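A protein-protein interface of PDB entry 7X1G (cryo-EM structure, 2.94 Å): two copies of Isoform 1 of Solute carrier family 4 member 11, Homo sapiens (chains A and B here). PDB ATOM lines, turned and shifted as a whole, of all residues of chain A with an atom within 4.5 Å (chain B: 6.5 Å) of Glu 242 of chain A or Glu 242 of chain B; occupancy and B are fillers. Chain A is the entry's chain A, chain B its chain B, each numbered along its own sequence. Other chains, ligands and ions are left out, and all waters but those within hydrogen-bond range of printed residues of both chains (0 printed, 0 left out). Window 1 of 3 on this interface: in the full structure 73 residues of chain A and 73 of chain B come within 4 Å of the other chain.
The side-chain amide oxygen (OE1) of Gln 199 of chain B sits close to the backbone carbonyl oxygen (O) of Asn 243 of chain B, at 3.5 Å. O of Glu 242 of chain B is in hydrogen-bond range of SG of Cys 245 of chain B (3.4 Å).
Of the 4 printed residues of chain A, 3 touch a printed residue of chain B. Along chain A the printed residues that touch a printed residue of chain B span positions 241 to 243. Printed residues of chain B that touch a printed residue of chain A: Tyr 210, Glu 242, Asn 243 and Pro 817. Among the printed residues, 5 pairs touch across the chains.
Glu 242 of chain A touches its own counterpart, Glu 242 of chain B. Glu 242 of chain A touches Asn 243 of chain B, and with the chains exchanged Asn 243 of chain A touches Glu 242 of chain B. Of the 5 pairs that touch across the chains among the printed residues, 3 have their exchanged pair printed and touching as well.
Among the printed residues, merely in contact across the chains: Glu 242 of chain A with Glu 242 of chain B, Gly 241 of chain A with Pro 817 of chain B, Glu 242 of chain A with Asn 243 of chain B, Asn 243 of chain A with Glu 242 of chain B and Glu 242 of chain A with Tyr 210 of chain B.
Of chain B, only Tyr 210 (3.9 Å), Glu 242 (3.2 Å) and Asn 243 (3.5 Å) come within 4 Å of Glu 242 of chain A. Glu 242 of chain B touches just these residues of chain A: Glu 242 (3.2 Å) and Asn 243 (3.8 Å). Of the printed residues of chain B, Gly 241 of chain A touches Pro 817. Of the printed residues of chain A, Asn 243 of chain B touches Glu 242. Arg 112 of chain B touches none of the printed residues of chain A. The nearest printed residue of chain A that does not touch Glu 242 of chain B is Gly 241 of chain A (6.7 Å). The nearest printed residue of chain A that does not touch Tyr 210 of chain B is Gly 241 of chain A (8.7 Å).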
ATOM      1  N   GLY A 241      -0.805  10.278 -22.553  1.00  0.00           N
ATOM      2  CA  GLY A 241       0.551  10.433 -23.029  1.00  0.00           C
ATOM      3  C   GLY A 241       1.086   9.116 -23.498  1.00  0.00           C
ATOM      4  O   GLY A 241       0.376   8.126 -23.486  1.00  0.00           O
ATOM      5  N   GLU A 242       2.339   9.080 -23.910  1.00  0.00           N
ATOM      6  CA  GLU A 242       2.943   7.818 -24.282  1.00  0.00           C
ATOM      7  C   GLU A 242       3.137   7.101 -22.971  1.00  0.00           C
ATOM      8  O   GLU A 242       3.443   7.749 -21.966  1.00  0.00           O
ATOM      9  CB  GLU A 242       4.292   8.039 -24.954  1.00  0.00           C
ATOM     10  CG  GLU A 242       4.316   9.158 -25.986  1.00  0.00           C
ATOM     11  CD  GLU A 242       4.775  10.487 -25.410  1.00  0.00           C
ATOM     12  OE1 GLU A 242       5.422  10.484 -24.341  1.00  0.00           O
ATOM     13  OE2 GLU A 242       4.495  11.535 -26.029  1.00  0.00           O
ATOM     14  N   ASN A 243       2.939   5.786 -22.961  1.00  0.00           N
ATOM     15  CA  ASN A 243       3.095   4.995 -21.745  1.00  0.00           C
ATOM     16  C   ASN A 243       2.089   5.402 -20.684  1.00  0.00           C
ATOM     17  O   ASN A 243       2.337   5.216 -19.500  1.00  0.00           O
ATOM     18  CB  ASN A 243       4.528   5.070 -21.241  1.00  0.00           C
ATOM     19  CG  ASN A 243       5.531   4.618 -22.282  1.00  0.00           C
ATOM     20  OD1 ASN A 243       5.260   3.712 -23.066  1.00  0.00           O
ATOM     21  ND2 ASN A 243       6.700   5.246 -22.290  1.00  0.00           N
ATOM     22  N   SER A 244       0.945   5.933 -21.103  1.00  0.00           N
ATOM     23  CA  SER A 244      -0.118   6.323 -20.187  1.00  0.00           C
ATOM     24  C   SER A 244      -1.339   6.392 -21.060  1.00  0.00           C
ATOM     25  O   SER A 244      -2.173   7.260 -20.883  1.00  0.00           O
ATOM     26  CB  SER A 244       0.148   7.679 -19.559  1.00  0.00           C
ATOM     27  OG  SER A 244       0.972   7.561 -18.417  1.00  0.00           O
ATOM     28  N   ARG B 112      10.345  16.507 -17.383  1.00  0.00           N
ATOM     29  CA  ARG B 112      10.465  17.139 -18.690  1.00  0.00           C
ATOM     30  C   ARG B 112      10.664  18.637 -18.516  1.00  0.00           C
ATOM     31  O   ARG B 112      10.035  19.261 -17.654  1.00  0.00           O
ATOM     32  CB  ARG B 112       9.224  16.870 -19.543  1.00  0.00           C
ATOM     33  CG  ARG B 112       9.306  15.591 -20.361  1.00  0.00           C
ATOM     34  CD  ARG B 112       7.994  14.826 -20.346  1.00  0.00           C
ATOM     35  NE  ARG B 112       8.150  13.471 -20.862  1.00  0.00           N
ATOM     36  CZ  ARG B 112       7.415  12.431 -20.489  1.00  0.00           C
ATOM     37  NH1 ARG B 112       6.442  12.552 -19.600  1.00  0.00           N
ATOM     38  NH2 ARG B 112       7.661  11.239 -21.024  1.00  0.00           N
ATOM     39  N   GLN B 199      16.052  15.544 -27.019  1.00  0.00           N
ATOM     40  CA  GLN B 199      15.477  15.235 -28.317  1.00  0.00           C
ATOM     41  C   GLN B 199      14.830  16.491 -28.881  1.00  0.00           C
ATOM     42  O   GLN B 199      14.543  17.445 -28.153  1.00  0.00           O
ATOM     43  CB  GLN B 199      14.429  14.120 -28.216  1.00  0.00           C
ATOM     44  CG  GLN B 199      14.980  12.764 -27.825  1.00  0.00           C
ATOM     45  CD  GLN B 199      13.896  11.712 -27.722  1.00  0.00           C
ATOM     46  OE1 GLN B 199      12.713  12.011 -27.879  1.00  0.00           O
ATOM     47  NE2 GLN B 199      14.290  10.475 -27.449  1.00  0.00           N
ATOM     48  N   VAL B 208       2.186  15.795 -30.351  1.00  0.00           N
ATOM     49  CA  VAL B 208       3.582  16.119 -30.084  1.00  0.00           C
ATOM     50  C   VAL B 208       4.441  15.172 -30.913  1.00  0.00           C
ATOM     51  O   VAL B 208       4.450  13.961 -30.678  1.00  0.00           O
ATOM     52  CB  VAL B 208       3.908  16.012 -28.590  1.00  0.00           C
ATOM     53  CG1 VAL B 208       5.410  16.047 -28.371  1.00  0.00           C
ATOM     54  CG2 VAL B 208       3.225  17.129 -27.818  1.00  0.00           C
ATOM     55  N   TYR B 210       8.089  13.978 -31.984  1.00  0.00           N
ATOM     56  CA  TYR B 210       9.485  13.973 -31.580  1.00  0.00           C
ATOM     57  C   TYR B 210      10.386  13.773 -32.790  1.00  0.00           C
ATOM     58  O   TYR B 210      10.026  13.090 -33.753  1.00  0.00           O
ATOM     59  CB  TYR B 210       9.750  12.869 -30.556  1.00  0.00           C
ATOM     60  CG  TYR B 210       9.316  13.207 -29.149  1.00  0.00           C
ATOM     61  CD1 TYR B 210       7.980  13.140 -28.778  1.00  0.00           C
ATOM     62  CD2 TYR B 210      10.243  13.591 -28.190  1.00  0.00           C
ATOM     63  CE1 TYR B 210       7.582  13.446 -27.491  1.00  0.00           C
ATOM     64  CE2 TYR B 210       9.853  13.900 -26.902  1.00  0.00           C
ATOM     65  CZ  TYR B 210       8.522  13.826 -26.559  1.00  0.00           C
ATOM     66  OH  TYR B 210       8.128  14.132 -25.277  1.00  0.00           O
ATOM     67  N   GLN B 212      12.936  11.768 -33.985  1.00  0.00           N
ATOM     68  CA  GLN B 212      13.431  10.449 -33.623  1.00  0.00           C
ATOM     69  C   GLN B 212      14.701  10.064 -34.368  1.00  0.00           C
ATOM     70  O   GLN B 212      15.195   8.949 -34.179  1.00  0.00           O
ATOM     71  CB  GLN B 212      12.348   9.397 -33.880  1.00  0.00           C
ATOM     72  CG  GLN B 212      10.937   9.873 -33.572  1.00  0.00           C
ATOM     73  CD  GLN B 212       9.913   8.762 -33.663  1.00  0.00           C
ATOM     74  OE1 GLN B 212      10.219   7.654 -34.100  1.00  0.00           O
ATOM     75  NE2 GLN B 212       8.686   9.054 -33.249  1.00  0.00           N
ATOM     76  N   ASN B 239      15.768   1.524 -33.004  1.00  0.00           N
ATOM     77  CA  ASN B 239      14.852   1.969 -31.956  1.00  0.00           C
ATOM     78  C   ASN B 239      15.729   2.166 -30.776  1.00  0.00           C
ATOM     79  O   ASN B 239      16.660   1.451 -30.615  1.00  0.00           O
ATOM     80  CB  ASN B 239      13.873   0.851 -31.695  1.00  0.00           C
ATOM     81  CG  ASN B 239      12.610   1.274 -31.028  1.00  0.00           C
ATOM     82  OD1 ASN B 239      11.556   1.300 -31.637  1.00  0.00           O
ATOM     83  ND2 ASN B 239      12.686   1.507 -29.757  1.00  0.00           N
ATOM     84  N   TRP B 240      15.507   3.160 -29.948  1.00  0.00           N
ATOM     85  CA  TRP B 240      16.415   3.410 -28.865  1.00  0.00           C
ATOM     86  C   TRP B 240      15.528   3.922 -27.799  1.00  0.00           C
ATOM     87  O   TRP B 240      15.993   4.442 -26.808  1.00  0.00           O
ATOM     88  CB  TRP B 240      17.433   4.473 -29.232  1.00  0.00           C
ATOM     89  CG  TRP B 240      18.792   3.983 -29.557  1.00  0.00           C
ATOM     90  CD1 TRP B 240      19.145   3.162 -30.570  1.00  0.00           C
ATOM     91  CD2 TRP B 240      19.995   4.316 -28.880  1.00  0.00           C
ATOM     92  NE1 TRP B 240      20.488   2.930 -30.557  1.00  0.00           N
ATOM     93  CE2 TRP B 240      21.036   3.635 -29.524  1.00  0.00           C
ATOM     94  CE3 TRP B 240      20.292   5.111 -27.779  1.00  0.00           C
ATOM     95  CZ2 TRP B 240      22.346   3.726 -29.108  1.00  0.00           C
ATOM     96  CZ3 TRP B 240      21.587   5.191 -27.367  1.00  0.00           C
ATOM     97  CH2 TRP B 240      22.603   4.508 -28.027  1.00  0.00           C
ATOM     98  N   GLY B 241      14.229   3.776 -27.992  1.00  0.00           N
ATOM     99  CA  GLY B 241      13.288   4.262 -27.020  1.00  0.00           C
ATOM    100  C   GLY B 241      11.868   4.210 -27.457  1.00  0.00           C
ATOM    101  O   GLY B 241      11.477   3.327 -28.178  1.00  0.00           O
ATOM    102  N   GLU B 242      11.075   5.162 -27.006  1.00  0.00           N
ATOM    103  CA  GLU B 242       9.667   5.164 -27.331  1.00  0.00           C
ATOM    104  C   GLU B 242       9.455   6.231 -28.318  1.00  0.00           C
ATOM    105  O   GLU B 242       8.632   6.107 -29.218  1.00  0.00           O
ATOM    106  CB  GLU B 242       8.833   5.493 -26.113  1.00  0.00           C
ATOM    107  CG  GLU B 242       7.670   4.547 -25.900  1.00  0.00           C
ATOM    108  CD  GLU B 242       6.481   4.904 -26.758  1.00  0.00           C
ATOM    109  OE1 GLU B 242       6.111   6.087 -26.770  1.00  0.00           O
ATOM    110  OE2 GLU B 242       5.925   4.007 -27.424  1.00  0.00           O
ATOM    111  N   ASN B 243      10.176   7.317 -28.146  1.00  0.00           N
ATOM    112  CA  ASN B 243      10.102   8.358 -29.115  1.00  0.00           C
ATOM    113  C   ASN B 243      11.473   8.423 -29.718  1.00  0.00           C
ATOM    114  O   ASN B 243      11.904   9.483 -30.125  1.00  0.00           O
ATOM    115  CB  ASN B 243       9.690   9.615 -28.435  1.00  0.00           C
ATOM    116  CG  ASN B 243       8.205   9.642 -28.137  1.00  0.00           C
ATOM    117  OD1 ASN B 243       7.382   9.429 -29.023  1.00  0.00           O
ATOM    118  ND2 ASN B 243       7.856   9.895 -26.885  1.00  0.00           N
ATOM    119  N   SER B 244      12.185   7.293 -29.735  1.00  0.00           N
ATOM    120  CA  SER B 244      13.476   7.245 -30.411  1.00  0.00           C
ATOM    121  C   SER B 244      13.551   6.011 -31.299  1.00  0.00           C
ATOM    122  O   SER B 244      14.531   5.262 -31.295  1.00  0.00           O
ATOM    123  CB  SER B 244      14.606   7.253 -29.387  1.00  0.00           C
ATOM    124  OG  SER B 244      14.773   8.540 -28.820  1.00  0.00           O
ATOM    125  N   CYS B 245      12.496   5.787 -32.082  1.00  0.00           N
ATOM    126  CA  CYS B 245      12.353   4.558 -32.850  1.00  0.00           C
ATOM    127  C   CYS B 245      13.239   4.506 -34.088  1.00  0.00           C
ATOM    128  O   CYS B 245      13.437   3.416 -34.635  1.00  0.00           O
ATOM    129  CB  CYS B 245      10.892   4.375 -33.266  1.00  0.00           C
ATOM    130  SG  CYS B 245       9.733   4.315 -31.881  1.00  0.00           S
ATOM    131  N   VAL B 739       7.909   6.948 -36.281  1.00  0.00           N
ATOM    132  CA  VAL B 739       7.005   5.905 -35.810  1.00  0.00           C
ATOM    133  C   VAL B 739       6.062   6.546 -34.800  1.00  0.00           C
ATOM    134  O   VAL B 739       6.443   6.811 -33.655  1.00  0.00           O
ATOM    135  CB  VAL B 739       7.764   4.723 -35.197  1.00  0.00           C
ATOM    136  CG1 VAL B 739       6.790   3.656 -34.723  1.00  0.00           C
ATOM    137  CG2 VAL B 739       8.747   4.145 -36.203  1.00  0.00           C
ATOM    138  N   PRO B 817      -2.869  13.082 -26.319  1.00  0.00           N
ATOM    139  CA  PRO B 817      -3.416  14.181 -25.506  1.00  0.00           C
ATOM    140  C   PRO B 817      -3.538  15.494 -26.260  1.00  0.00           C
ATOM    141  O   PRO B 817      -4.498  16.242 -26.039  1.00  0.00           O
ATOM    142  CB  PRO B 817      -2.416  14.289 -24.344  1.00  0.00           C
ATOM    143  CG  PRO B 817      -1.706  12.985 -24.313  1.00  0.00           C
ATOM    144  CD  PRO B 817      -1.646  12.515 -25.726  1.00  0.00           C
